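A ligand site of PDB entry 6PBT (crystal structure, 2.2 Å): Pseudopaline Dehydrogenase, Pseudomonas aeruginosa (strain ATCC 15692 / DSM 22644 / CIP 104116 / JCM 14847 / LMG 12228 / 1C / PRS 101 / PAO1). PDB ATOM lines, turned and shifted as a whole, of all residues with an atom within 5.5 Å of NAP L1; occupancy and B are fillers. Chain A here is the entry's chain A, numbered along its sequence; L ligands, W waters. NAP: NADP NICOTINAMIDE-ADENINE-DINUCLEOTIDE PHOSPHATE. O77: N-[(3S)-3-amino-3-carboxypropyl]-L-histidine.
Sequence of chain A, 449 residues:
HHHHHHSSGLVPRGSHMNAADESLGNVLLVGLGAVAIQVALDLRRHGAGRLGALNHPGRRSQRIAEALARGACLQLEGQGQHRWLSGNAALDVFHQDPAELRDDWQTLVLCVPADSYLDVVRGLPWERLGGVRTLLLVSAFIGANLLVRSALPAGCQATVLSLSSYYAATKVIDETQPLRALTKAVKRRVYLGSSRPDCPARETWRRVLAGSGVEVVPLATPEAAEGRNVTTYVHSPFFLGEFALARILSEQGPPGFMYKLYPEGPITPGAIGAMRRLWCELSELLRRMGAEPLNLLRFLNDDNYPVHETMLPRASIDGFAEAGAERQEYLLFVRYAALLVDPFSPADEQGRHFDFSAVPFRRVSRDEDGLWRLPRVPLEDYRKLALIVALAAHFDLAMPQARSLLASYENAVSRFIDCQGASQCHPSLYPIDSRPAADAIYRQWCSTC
The backbone carbonyl oxygen of Asn 55 lies within hydrogen-bond range of the side-chain hydroxyl of Ser 61 (3.0 Å).
NE of Arg 376 lies within salt-bridge range of OE2 of Glu 380 (3.7 Å).
The backbone carbonyl oxygen (O) of Tyr 166 is in hydrogen-bond range of the side-chain amino group (NZ) of Lys 187.
The side-chain carboxylate of Glu 380 sits at hydrogen-bond distance from the backbone NH of Ala 114 (3.5 Å).
The backbone carbonyl oxygen of His 56 lies within hydrogen-bond range of the side-chain hydroxyl of Ser 61, 2.8 Å away.
The backbone carbonyl oxygen (O) of Leu 32 sits at hydrogen-bond distance from the guanidinium group (NH1) of Arg 60.
The side-chain hydroxyl (OH) of Tyr 166 is in hydrogen-bond range of the side-chain hydroxyl (OG1) of Thr 170.
N of Leu 32 sits at hydrogen-bond distance from OD1 of Asn 55 (3.0 Å).
An oxygen (O3B) of NAP L1 lies close to the backbone carbonyl oxygen of Leu 32, at 3.3 Å.
The backbone NH of Ala 34 is in hydrogen-bond range of an oxygen (O2N) of NAP L1 (3.2 Å).
An oxygen (O3X) of NAP L1 sits at hydrogen-bond distance from a ring nitrogen (NE2) of His 56.
A nitrogen (N7N) of NAP L1 lies within hydrogen-bond range of the backbone carbonyl oxygen of Thr 170, 3.0 Å away.
The guanidinium group (NH2) of Arg 376 is in salt-bridge range of an oxygen (O2A) of NAP L1 (2.8 Å).
NZ of Lys 187 lies within salt-bridge range of O16 of O77 L2 (3.9 Å).
N of Thr 170 sits at hydrogen-bond distance from O7N of NAP L1 (3.0 Å).
An oxygen (O2D) of NAP L1 sits at hydrogen-bond distance from the backbone NH (N) of Ala 114 (3.5 Å).
An oxygen (O2D) of NAP L1 sits at hydrogen-bond distance from the side-chain carboxylate (OE1) of Glu 380 (2.6 Å).
An oxygen (O3B) of NAP L1 sits at hydrogen-bond distance from the backbone NH of Leu 32, at 3.1 Å.
The backbone NH (N) of Gly 33 lies within hydrogen-bond range of an oxygen (O3B) of NAP L1.
An oxygen (O3B) of NAP L1 is in hydrogen-bond range of the side-chain amide oxygen (OD1) of Asn 55.
NE of Arg 60 lies within hydrogen-bond range of O3B of NAP L1 (3.5 Å).
N of Val 35 sits at hydrogen-bond distance from O2N of NAP L1 (2.9 Å).
Water W5 lies within hydrogen-bond range of an oxygen (O2X) of NAP L1 (2.9 Å) and the backbone NH (N) of Arg 60 (3.0 Å).
Water W1 bridges the side-chain carboxylate of Asp 119 (2.9 Å) and a nitrogen (N6A) of NAP L1 (3.0 Å).
Gly 31 touches NAP L1.
O of Cys 111 touches C5D of NAP L1 (3.7 Å).
CG1 of Val 112 touches N3A of NAP L1, 3.7 Å away.
Pro 113 touches NAP L1 (CA to O3D, 3.2 Å).
Ser 116 touches NAP L1.
CG2 of Val 120 touches C2A of NAP L1 (3.7 Å).
Ser 139 touches NAP L1.
Tyr 166 touches NAP L1.
Ala 168 touches NAP L1.
Ala 169 touches NAP L1.
Hydrophobic or aromatic side chains within 4 Å of NAP L1: Ala 34, Val 35, His 56, Val 112, Pro 113, Val 120 and Tyr 166.
The nearest printed residue that does not touch NAP L1 is Ala 36 (4.6 Å).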
ATOM      1  N   GLY A  31     -11.772   2.228   5.200  1.00  0.00           N
ATOM      2  CA  GLY A  31     -11.523   3.384   4.389  1.00  0.00           C
ATOM      3  C   GLY A  31     -10.355   3.039   3.540  1.00  0.00           C
ATOM      4  O   GLY A  31      -9.344   2.866   4.033  1.00  0.00           O
ATOM      5  N   LEU A  32     -10.505   2.919   2.252  1.00  0.00           N
ATOM      6  CA  LEU A  32      -9.419   2.533   1.424  1.00  0.00           C
ATOM      7  C   LEU A  32      -8.809   3.636   0.583  1.00  0.00           C
ATOM      8  O   LEU A  32      -8.974   3.650  -0.573  1.00  0.00           O
ATOM      9  CB  LEU A  32      -9.889   1.431   0.513  1.00  0.00           C
ATOM     10  CG  LEU A  32      -8.947   0.342   0.153  1.00  0.00           C
ATOM     11  CD1 LEU A  32      -9.483  -0.541  -0.916  1.00  0.00           C
ATOM     12  CD2 LEU A  32      -7.571   0.731  -0.152  1.00  0.00           C
ATOM     13  N   GLY A  33      -8.079   4.522   1.219  1.00  0.00           N
ATOM     14  CA  GLY A  33      -7.453   5.635   0.569  1.00  0.00           C
ATOM     15  C   GLY A  33      -5.955   5.564   0.521  1.00  0.00           C
ATOM     16  O   GLY A  33      -5.420   4.533   0.614  1.00  0.00           O
ATOM     17  N   ALA A  34      -5.302   6.714   0.395  1.00  0.00           N
ATOM     18  CA  ALA A  34      -3.851   6.758   0.327  1.00  0.00           C
ATOM     19  C   ALA A  34      -3.222   6.116   1.553  1.00  0.00           C
ATOM     20  O   ALA A  34      -2.317   5.285   1.437  1.00  0.00           O
ATOM     21  CB  ALA A  34      -3.404   8.209   0.194  1.00  0.00           C
ATOM     22  N   VAL A  35      -3.704   6.471   2.747  1.00  0.00           N
ATOM     23  CA  VAL A  35      -3.133   5.912   3.968  1.00  0.00           C
ATOM     24  C   VAL A  35      -3.290   4.407   3.975  1.00  0.00           C
ATOM     25  O   VAL A  35      -2.367   3.663   4.282  1.00  0.00           O
ATOM     26  CB  VAL A  35      -3.798   6.545   5.201  1.00  0.00           C
ATOM     27  CG1 VAL A  35      -3.501   5.754   6.459  1.00  0.00           C
ATOM     28  CG2 VAL A  35      -3.328   7.946   5.391  1.00  0.00           C
ATOM     29  N   ALA A  36      -4.492   3.923   3.646  1.00  0.00           N
ATOM     30  CA  ALA A  36      -4.726   2.494   3.698  1.00  0.00           C
ATOM     31  C   ALA A  36      -3.739   1.743   2.816  1.00  0.00           C
ATOM     32  O   ALA A  36      -3.410   0.583   3.096  1.00  0.00           O
ATOM     33  CB  ALA A  36      -6.183   2.163   3.300  1.00  0.00           C
ATOM     34  N   ASN A  55     -15.012   0.248   2.390  1.00  0.00           N
ATOM     35  CA  ASN A  55     -15.149   1.656   2.045  1.00  0.00           C
ATOM     36  C   ASN A  55     -16.609   1.992   1.702  1.00  0.00           C
ATOM     37  O   ASN A  55     -17.237   1.297   0.903  1.00  0.00           O
ATOM     38  CB  ASN A  55     -14.262   1.982   0.878  1.00  0.00           C
ATOM     39  CG  ASN A  55     -13.929   3.477   0.793  1.00  0.00           C
ATOM     40  OD1 ASN A  55     -13.259   4.036   1.664  1.00  0.00           O
ATOM     41  ND2 ASN A  55     -14.436   4.129  -0.245  1.00  0.00           N
ATOM     42  N   HIS A  56     -17.133   3.058   2.273  1.00  0.00           N
ATOM     43  CA  HIS A  56     -18.558   3.335   2.093  1.00  0.00           C
ATOM     44  C   HIS A  56     -18.868   3.602   0.618  1.00  0.00           C
ATOM     45  O   HIS A  56     -17.974   3.887  -0.178  1.00  0.00           O
ATOM     46  CB  HIS A  56     -19.029   4.484   2.980  1.00  0.00           C
ATOM     47  CG  HIS A  56     -18.415   5.838   2.710  1.00  0.00           C
ATOM     48  ND1 HIS A  56     -18.818   6.956   3.413  1.00  0.00           N
ATOM     49  CD2 HIS A  56     -17.458   6.260   1.848  1.00  0.00           C
ATOM     50  CE1 HIS A  56     -18.116   7.999   3.011  1.00  0.00           C
ATOM     51  NE2 HIS A  56     -17.285   7.609   2.067  1.00  0.00           N
ATOM     52  N   PRO A  57     -20.125   3.392   0.225  1.00  0.00           N
ATOM     53  CA  PRO A  57     -20.453   3.423  -1.207  1.00  0.00           C
ATOM     54  C   PRO A  57     -20.191   4.796  -1.795  1.00  0.00           C
ATOM     55  O   PRO A  57     -20.215   5.824  -1.116  1.00  0.00           O
ATOM     56  CB  PRO A  57     -21.953   3.061  -1.238  1.00  0.00           C
ATOM     57  CG  PRO A  57     -22.288   2.460   0.105  1.00  0.00           C
ATOM     58  CD  PRO A  57     -21.283   3.035   1.076  1.00  0.00           C
ATOM     59  N   GLY A  58     -19.941   4.810  -3.088  1.00  0.00           N
ATOM     60  CA  GLY A  58     -19.563   6.058  -3.732  1.00  0.00           C
ATOM     61  C   GLY A  58     -18.697   5.792  -4.945  1.00  0.00           C
ATOM     62  O   GLY A  58     -18.390   4.671  -5.310  1.00  0.00           O
ATOM     63  N   ARG A  59     -18.288   6.898  -5.567  1.00  0.00           N
ATOM     64  CA  ARG A  59     -17.507   6.838  -6.785  1.00  0.00           C
ATOM     65  C   ARG A  59     -16.184   6.128  -6.579  1.00  0.00           C
ATOM     66  O   ARG A  59     -15.758   5.326  -7.417  1.00  0.00           O
ATOM     67  CB  ARG A  59     -17.263   8.251  -7.299  1.00  0.00           C
ATOM     68  CG  ARG A  59     -17.242   8.333  -8.788  1.00  0.00           C
ATOM     69  CD  ARG A  59     -17.024   9.777  -9.299  1.00  0.00           C
ATOM     70  NE  ARG A  59     -17.036   9.731 -10.751  1.00  0.00           N
ATOM     71  CZ  ARG A  59     -18.145   9.784 -11.486  1.00  0.00           C
ATOM     72  NH1 ARG A  59     -19.335   9.936 -10.904  1.00  0.00           N
ATOM     73  NH2 ARG A  59     -18.070   9.678 -12.812  1.00  0.00           N
ATOM     74  N   ARG A  60     -15.474   6.457  -5.489  1.00  0.00           N
ATOM     75  CA  ARG A  60     -14.193   5.783  -5.250  1.00  0.00           C
ATOM     76  C   ARG A  60     -14.392   4.280  -5.053  1.00  0.00           C
ATOM     77  O   ARG A  60     -13.678   3.468  -5.650  1.00  0.00           O
ATOM     78  CB  ARG A  60     -13.488   6.374  -4.026  1.00  0.00           C
ATOM     79  CG  ARG A  60     -12.048   5.830  -3.908  1.00  0.00           C
ATOM     80  CD  ARG A  60     -11.160   6.590  -2.910  1.00  0.00           C
ATOM     81  NE  ARG A  60     -10.111   5.664  -2.456  1.00  0.00           N
ATOM     82  CZ  ARG A  60      -9.000   5.366  -3.153  1.00  0.00           C
ATOM     83  NH1 ARG A  60      -8.125   4.506  -2.680  1.00  0.00           N
ATOM     84  NH2 ARG A  60      -8.756   5.964  -4.319  1.00  0.00           N
ATOM     85  N   SER A  61     -15.325   3.890  -4.205  1.00  0.00           N
ATOM     86  CA  SER A  61     -15.583   2.470  -4.004  1.00  0.00           C
ATOM     87  C   SER A  61     -15.895   1.786  -5.321  1.00  0.00           C
ATOM     88  O   SER A  61     -15.417   0.674  -5.585  1.00  0.00           O
ATOM     89  CB  SER A  61     -16.738   2.288  -3.027  1.00  0.00           C
ATOM     90  OG  SER A  61     -16.264   2.311  -1.694  1.00  0.00           O
ATOM     91  N   ILE A  64     -12.723   1.276  -7.215  1.00  0.00           N
ATOM     92  CA  ILE A  64     -11.915   0.246  -6.569  1.00  0.00           C
ATOM     93  C   ILE A  64     -12.402  -1.121  -6.978  1.00  0.00           C
ATOM     94  O   ILE A  64     -11.607  -1.982  -7.370  1.00  0.00           O
ATOM     95  CB  ILE A  64     -11.943   0.420  -5.037  1.00  0.00           C
ATOM     96  CG1 ILE A  64     -11.165   1.665  -4.623  1.00  0.00           C
ATOM     97  CG2 ILE A  64     -11.352  -0.829  -4.332  1.00  0.00           C
ATOM     98  CD1 ILE A  64     -11.393   2.068  -3.157  1.00  0.00           C
ATOM     99  N   CYS A 111      -8.505   3.982   8.500  1.00  0.00           N
ATOM    100  CA  CYS A 111      -7.738   4.790   7.579  1.00  0.00           C
ATOM    101  C   CYS A 111      -8.587   5.902   6.980  1.00  0.00           C
ATOM    102  O   CYS A 111      -8.234   6.458   5.939  1.00  0.00           O
ATOM    103  CB  CYS A 111      -7.158   3.897   6.490  1.00  0.00           C
ATOM    104  SG  CYS A 111      -6.161   2.510   7.149  1.00  0.00           S
ATOM    105  N   VAL A 112      -9.730   6.169   7.598  1.00  0.00           N
ATOM    106  CA  VAL A 112     -10.676   7.209   7.196  1.00  0.00           C
ATOM    107  C   VAL A 112     -10.183   8.536   7.782  1.00  0.00           C
ATOM    108  O   VAL A 112      -9.371   8.521   8.726  1.00  0.00           O
ATOM    109  CB  VAL A 112     -12.103   6.892   7.679  1.00  0.00           C
ATOM    110  CG1 VAL A 112     -12.666   5.643   7.046  1.00  0.00           C
ATOM    111  CG2 VAL A 112     -12.144   6.759   9.204  1.00  0.00           C
ATOM    112  N   PRO A 113     -10.655   9.679   7.303  1.00  0.00           N
ATOM    113  CA  PRO A 113     -10.336  10.939   7.980  1.00  0.00           C
ATOM    114  C   PRO A 113     -10.696  10.868   9.466  1.00  0.00           C
ATOM    115  O   PRO A 113     -11.694  10.291   9.862  1.00  0.00           O
ATOM    116  CB  PRO A 113     -11.194  11.976   7.249  1.00  0.00           C
ATOM    117  CG  PRO A 113     -11.619  11.313   5.922  1.00  0.00           C
ATOM    118  CD  PRO A 113     -11.691   9.841   6.263  1.00  0.00           C
ATOM    119  N   ALA A 114      -9.861  11.492  10.288  1.00  0.00           N
ATOM    120  CA  ALA A 114     -10.039  11.343  11.726  1.00  0.00           C
ATOM    121  C   ALA A 114     -11.319  11.977  12.222  1.00  0.00           C
ATOM    122  O   ALA A 114     -11.826  11.568  13.263  1.00  0.00           O
ATOM    123  CB  ALA A 114      -8.836  11.965  12.470  1.00  0.00           C
ATOM    124  N   SER A 116     -14.130  11.697  10.943  1.00  0.00           N
ATOM    125  CA  SER A 116     -15.179  10.718  10.696  1.00  0.00           C
ATOM    126  C   SER A 116     -15.105   9.485  11.589  1.00  0.00           C
ATOM    127  O   SER A 116     -15.906   8.560  11.400  1.00  0.00           O
ATOM    128  CB  SER A 116     -15.109  10.285   9.235  1.00  0.00           C
ATOM    129  OG  SER A 116     -14.098   9.297   9.077  1.00  0.00           O
ATOM    130  N   ASP A 119     -18.517   8.632  13.292  1.00  0.00           N
ATOM    131  CA  ASP A 119     -19.509   8.090  12.357  1.00  0.00           C
ATOM    132  C   ASP A 119     -19.155   6.666  11.949  1.00  0.00           C
ATOM    133  O   ASP A 119     -20.008   5.794  11.851  1.00  0.00           O
ATOM    134  CB  ASP A 119     -19.604   8.938  11.104  1.00  0.00           C
ATOM    135  CG  ASP A 119     -20.277  10.291  11.351  1.00  0.00           C
ATOM    136  OD1 ASP A 119     -20.904  10.484  12.428  1.00  0.00           O
ATOM    137  OD2 ASP A 119     -20.170  11.145  10.454  1.00  0.00           O
ATOM    138  N   VAL A 120     -17.877   6.434  11.658  1.00  0.00           N
ATOM    139  CA  VAL A 120     -17.449   5.146  11.133  1.00  0.00           C
ATOM    140  C   VAL A 120     -17.589   4.065  12.182  1.00  0.00           C
ATOM    141  O   VAL A 120     -18.025   2.954  11.882  1.00  0.00           O
ATOM    142  CB  VAL A 120     -15.998   5.264  10.629  1.00  0.00           C
ATOM    143  CG1 VAL A 120     -15.327   3.926  10.542  1.00  0.00           C
ATOM    144  CG2 VAL A 120     -15.975   5.968   9.283  1.00  0.00           C
ATOM    145  N   SER A 139      -4.551   8.118  12.660  1.00  0.00           N
ATOM    146  CA  SER A 139      -4.292   9.534  12.835  1.00  0.00           C
ATOM    147  C   SER A 139      -5.183  10.083  13.965  1.00  0.00           C
ATOM    148  O   SER A 139      -6.173  10.772  13.742  1.00  0.00           O
ATOM    149  CB  SER A 139      -4.559  10.302  11.532  1.00  0.00           C
ATOM    150  OG  SER A 139      -4.027  11.594  11.640  1.00  0.00           O
ATOM    151  N   TYR A 166      -0.366   9.946  11.187  1.00  0.00           N
ATOM    152  CA  TYR A 166       0.020   9.093  10.070  1.00  0.00           C
ATOM    153  C   TYR A 166       1.509   9.309   9.818  1.00  0.00           C
ATOM    154  O   TYR A 166       2.005  10.425   9.879  1.00  0.00           O
ATOM    155  CB  TYR A 166      -0.807   9.427   8.836  1.00  0.00           C
ATOM    156  CG  TYR A 166      -0.363   8.684   7.615  1.00  0.00           C
ATOM    157  CD1 TYR A 166      -0.290   7.309   7.607  1.00  0.00           C
ATOM    158  CD2 TYR A 166       0.021   9.367   6.466  1.00  0.00           C
ATOM    159  CE1 TYR A 166       0.123   6.639   6.475  1.00  0.00           C
ATOM    160  CE2 TYR A 166       0.442   8.687   5.326  1.00  0.00           C
ATOM    161  CZ  TYR A 166       0.500   7.331   5.345  1.00  0.00           C
ATOM    162  OH  TYR A 166       0.892   6.655   4.212  1.00  0.00           O
ATOM    163  N   ALA A 168       3.540   9.113   7.290  1.00  0.00           N
ATOM    164  CA  ALA A 168       4.121   9.385   5.981  1.00  0.00           C
ATOM    165  C   ALA A 168       3.364  10.523   5.312  1.00  0.00           C
ATOM    166  O   ALA A 168       2.524  11.177   5.934  1.00  0.00           O
ATOM    167  CB  ALA A 168       4.090   8.101   5.133  1.00  0.00           C
ATOM    168  N   ALA A 169       3.708  10.800   4.058  1.00  0.00           N
ATOM    169  CA  ALA A 169       2.948  11.731   3.237  1.00  0.00           C
ATOM    170  C   ALA A 169       2.644  10.992   1.939  1.00  0.00           C
ATOM    171  O   ALA A 169       3.542  10.719   1.154  1.00  0.00           O
ATOM    172  CB  ALA A 169       3.733  13.028   3.006  1.00  0.00           C
ATOM    173  N   THR A 170       1.381  10.605   1.764  1.00  0.00           N
ATOM    174  CA  THR A 170       0.973   9.711   0.684  1.00  0.00           C
ATOM    175  C   THR A 170      -0.254  10.307   0.025  1.00  0.00           C
ATOM    176  O   THR A 170      -1.117  10.883   0.697  1.00  0.00           O
ATOM    177  CB  THR A 170       0.658   8.319   1.202  1.00  0.00           C
ATOM    178  OG1 THR A 170       1.638   7.972   2.174  1.00  0.00           O
ATOM    179  CG2 THR A 170       0.677   7.295   0.096  1.00  0.00           C
ATOM    180  N   LYS A 171      -0.327  10.126  -1.300  1.00  0.00           N
ATOM    181  CA  LYS A 171      -1.413  10.621  -2.138  1.00  0.00           C
ATOM    182  C   LYS A 171      -1.753   9.587  -3.204  1.00  0.00           C
ATOM    183  O   LYS A 171      -0.856   8.877  -3.692  1.00  0.00           O
ATOM    184  CB  LYS A 171      -1.009  11.929  -2.800  1.00  0.00           C
ATOM    185  CG  LYS A 171      -2.114  12.947  -2.885  1.00  0.00           C
ATOM    186  CD  LYS A 171      -2.556  13.186  -4.325  1.00  0.00           C
ATOM    187  CE  LYS A 171      -3.652  14.256  -4.397  1.00  0.00           C
ATOM    188  NZ  LYS A 171      -4.558  14.102  -5.575  1.00  0.00           N
ATOM    189  N   VAL A 172      -3.031   9.468  -3.530  1.00  0.00           N
ATOM    190  CA  VAL A 172      -3.450   8.717  -4.712  1.00  0.00           C
ATOM    191  C   VAL A 172      -3.191   9.603  -5.908  1.00  0.00           C
ATOM    192  O   VAL A 172      -3.786  10.685  -6.022  1.00  0.00           O
ATOM    193  CB  VAL A 172      -4.925   8.303  -4.643  1.00  0.00           C
ATOM    194  CG1 VAL A 172      -5.396   7.753  -6.009  1.00  0.00           C
ATOM    195  CG2 VAL A 172      -5.155   7.248  -3.612  1.00  0.00           C
ATOM    196  N   LYS A 187       7.955  10.001   8.166  1.00  0.00           N
ATOM    197  CA  LYS A 187       8.373  10.664   9.391  1.00  0.00           C
ATOM    198  C   LYS A 187       9.510   9.879  10.032  1.00  0.00           C
ATOM    199  O   LYS A 187       9.651   8.673   9.832  1.00  0.00           O
ATOM    200  CB  LYS A 187       7.184  10.810  10.339  1.00  0.00           C
ATOM    201  CG  LYS A 187       6.298  12.027   9.954  1.00  0.00           C
ATOM    202  CD  LYS A 187       5.039  11.997  10.740  1.00  0.00           C
ATOM    203  CE  LYS A 187       4.154  13.169  10.393  1.00  0.00           C
ATOM    204  NZ  LYS A 187       3.305  12.887   9.196  1.00  0.00           N
ATOM    205  N   THR A 231      -0.473  17.586  13.207  1.00  0.00           N
ATOM    206  CA  THR A 231      -1.310  18.520  12.462  1.00  0.00           C
ATOM    207  C   THR A 231      -2.092  19.437  13.414  1.00  0.00           C
ATOM    208  O   THR A 231      -2.351  20.604  13.065  1.00  0.00           O
ATOM    209  CB  THR A 231      -2.295  17.831  11.508  1.00  0.00           C
ATOM    210  OG1 THR A 231      -3.199  16.999  12.231  1.00  0.00           O
ATOM    211  CG2 THR A 231      -1.544  16.962  10.528  1.00  0.00           C
ATOM    212  N   ARG A 376     -10.167  19.067   2.990  1.00  0.00           N
ATOM    213  CA  ARG A 376      -9.902  18.503   4.314  1.00  0.00           C
ATOM    214  C   ARG A 376      -9.021  19.429   5.165  1.00  0.00           C
ATOM    215  O   ARG A 376      -9.230  19.531   6.383  1.00  0.00           O
ATOM    216  CB  ARG A 376      -9.276  17.131   4.117  1.00  0.00           C
ATOM    217  CG  ARG A 376      -8.393  16.662   5.233  1.00  0.00           C
ATOM    218  CD  ARG A 376      -7.948  15.234   4.942  1.00  0.00           C
ATOM    219  NE  ARG A 376      -8.999  14.427   4.285  1.00  0.00           N
ATOM    220  CZ  ARG A 376      -8.758  13.453   3.399  1.00  0.00           C
ATOM    221  NH1 ARG A 376      -7.495  13.157   3.055  1.00  0.00           N
ATOM    222  NH2 ARG A 376      -9.757  12.792   2.846  1.00  0.00           N
ATOM    223  N   GLU A 380     -11.104  19.302   8.314  1.00  0.00           N
ATOM    224  CA  GLU A 380     -10.724  18.319   9.321  1.00  0.00           C
ATOM    225  C   GLU A 380     -10.056  18.981  10.522  1.00  0.00           C
ATOM    226  O   GLU A 380     -10.346  18.650  11.676  1.00  0.00           O
ATOM    227  CB  GLU A 380      -9.790  17.266   8.713  1.00  0.00           C
ATOM    228  CG  GLU A 380      -9.559  16.132   9.682  1.00  0.00           C
ATOM    229  CD  GLU A 380      -8.623  15.005   9.155  1.00  0.00           C
ATOM    230  OE1 GLU A 380      -7.941  14.396   9.985  1.00  0.00           O
ATOM    231  OE2 GLU A 380      -8.582  14.732   7.952  1.00  0.00           O
HETATM  232  PA  NAP L   1      -8.363   9.657   1.425  1.00  0.00           P
HETATM  233  O1A NAP L   1      -7.522   9.233   0.395  1.00  0.00           O
HETATM  234  O2A NAP L   1      -9.323  10.595   1.107  1.00  0.00           O
HETATM  235  O5B NAP L   1      -9.039   8.360   1.916  1.00  0.00           O
HETATM  236  C5B NAP L   1      -9.938   8.127   2.927  1.00  0.00           C
HETATM  237  C4B NAP L   1     -10.784   6.923   2.614  1.00  0.00           C
HETATM  238  O4B NAP L   1     -11.844   6.959   3.463  1.00  0.00           O
HETATM  239  C3B NAP L   1     -11.381   6.902   1.223  1.00  0.00           C
HETATM  240  O3B NAP L   1     -11.318   5.587   0.821  1.00  0.00           O
HETATM  241  C2B NAP L   1     -12.740   7.513   1.413  1.00  0.00           C
HETATM  242  O2B NAP L   1     -13.678   7.197   0.439  1.00  0.00           O
HETATM  243  C1B NAP L   1     -13.065   7.135   2.825  1.00  0.00           C
HETATM  244  N9A NAP L   1     -13.809   8.159   3.541  1.00  0.00           N
HETATM  245  C8A NAP L   1     -13.659   9.450   3.433  1.00  0.00           C
HETATM  246  N7A NAP L   1     -14.516  10.044   4.234  1.00  0.00           N
HETATM  247  C5A NAP L   1     -15.265   9.163   4.842  1.00  0.00           C
HETATM  248  C6A NAP L   1     -16.373   9.156   5.817  1.00  0.00           C
HETATM  249  N6A NAP L   1     -16.888  10.283   6.319  1.00  0.00           N
HETATM  250  N1A NAP L   1     -16.846   7.982   6.171  1.00  0.00           N
HETATM  251  C2A NAP L   1     -16.346   6.875   5.705  1.00  0.00           C
HETATM  252  N3A NAP L   1     -15.369   6.843   4.840  1.00  0.00           N
HETATM  253  C4A NAP L   1     -14.788   7.915   4.376  1.00  0.00           C
HETATM  254  O3  NAP L   1      -7.557  10.099   2.667  1.00  0.00           O
HETATM  255  PN  NAP L   1      -6.114   9.696   3.079  1.00  0.00           P
HETATM  256  O1N NAP L   1      -5.281  10.532   2.351  1.00  0.00           O
HETATM  257  O2N NAP L   1      -5.896   8.309   3.112  1.00  0.00           O
HETATM  258  O5D NAP L   1      -6.046  10.375   4.432  1.00  0.00           O
HETATM  259  C5D NAP L   1      -6.705   9.854   5.509  1.00  0.00           C
HETATM  260  C4D NAP L   1      -6.492  10.590   6.782  1.00  0.00           C
HETATM  261  O4D NAP L   1      -5.229  10.388   7.306  1.00  0.00           O
HETATM  262  C3D NAP L   1      -6.604  12.077   6.650  1.00  0.00           C
HETATM  263  O3D NAP L   1      -7.924  12.521   6.645  1.00  0.00           O
HETATM  264  C2D NAP L   1      -5.910  12.510   7.866  1.00  0.00           C
HETATM  265  O2D NAP L   1      -6.742  12.332   8.994  1.00  0.00           O
HETATM  266  C1D NAP L   1      -4.768  11.553   7.894  1.00  0.00           C
HETATM  267  N1N NAP L   1      -3.564  12.070   7.236  1.00  0.00           N
HETATM  268  C2N NAP L   1      -3.217  11.701   6.026  1.00  0.00           C
HETATM  269  C3N NAP L   1      -2.084  12.168   5.431  1.00  0.00           C
HETATM  270  C7N NAP L   1      -1.701  11.729   4.051  1.00  0.00           C
HETATM  271  O7N NAP L   1      -0.597  11.801   3.684  1.00  0.00           O
HETATM  272  N7N NAP L   1      -2.596  11.225   3.289  1.00  0.00           N
HETATM  273  C4N NAP L   1      -1.260  13.043   6.145  1.00  0.00           C
HETATM  274  C5N NAP L   1      -1.662  13.386   7.396  1.00  0.00           C
HETATM  275  C6N NAP L   1      -2.807  12.868   7.926  1.00  0.00           C
HETATM  276  P2B NAP L   1     -14.482   8.307  -0.300  1.00  0.00           P
HETATM  277  O1X NAP L   1     -13.597   9.101  -0.998  1.00  0.00           O
HETATM  278  O2X NAP L   1     -15.293   7.625  -1.111  1.00  0.00           O
HETATM  279  O3X NAP L   1     -15.168   8.936   0.740  1.00  0.00           O
HETATM  280  C02 O77 L   2       5.940  21.038   9.521  1.00  0.00           C
HETATM  281  C03 O77 L   2       5.802  20.305   8.212  1.00  0.00           C
HETATM  282  C04 O77 L   2       6.386  21.370   7.293  1.00  0.00           C
HETATM  283  C05 O77 L   2       6.258  21.166   5.827  1.00  0.00           C
HETATM  284  C06 O77 L   2       5.688  20.124   5.183  1.00  0.00           C
HETATM  285  C08 O77 L   2       6.470  21.509   3.795  1.00  0.00           C
HETATM  286  C11 O77 L   2       3.787  19.397   9.109  1.00  0.00           C
HETATM  287  C12 O77 L   2       2.363  19.044   8.727  1.00  0.00           C
HETATM  288  C13 O77 L   2       2.354  17.795   7.886  1.00  0.00           C
HETATM  289  C15 O77 L   2       1.086  17.064   8.156  1.00  0.00           C
HETATM  290  N07 O77 L   2       5.832  20.388   3.929  1.00  0.00           N
HETATM  291  N09 O77 L   2       6.723  21.974   4.948  1.00  0.00           N
HETATM  292  N10 O77 L   2       4.427  20.030   8.004  1.00  0.00           N
HETATM  293  N14 O77 L   2       2.410  18.058   6.474  1.00  0.00           N
HETATM  294  O01 O77 L   2       5.166  21.889   9.906  1.00  0.00           O
HETATM  295  O16 O77 L   2       1.123  16.060   8.882  1.00  0.00           O
HETATM  296  O17 O77 L   2       0.056  17.438   7.612  1.00  0.00           O
HETATM  297  O18 O77 L   2       6.880  20.717  10.193  1.00  0.00           O
HETATM  298  O   HOH W   1     -19.503  10.150   7.866  1.00  0.00           O
HETATM  299  O   HOH W   2     -16.705   5.546  -2.254  1.00  0.00           O
HETATM  300  O   HOH W   3      -6.986   5.864   3.562  1.00  0.00           O
HETATM  301  O   HOH W   4      -4.611  11.752   0.291  1.00  0.00           O
HETATM  302  O   HOH W   5     -15.855   8.766  -3.692  1.00  0.00           O
HETATM  303  O   HOH W   6     -19.408   7.640   7.590  1.00  0.00           O
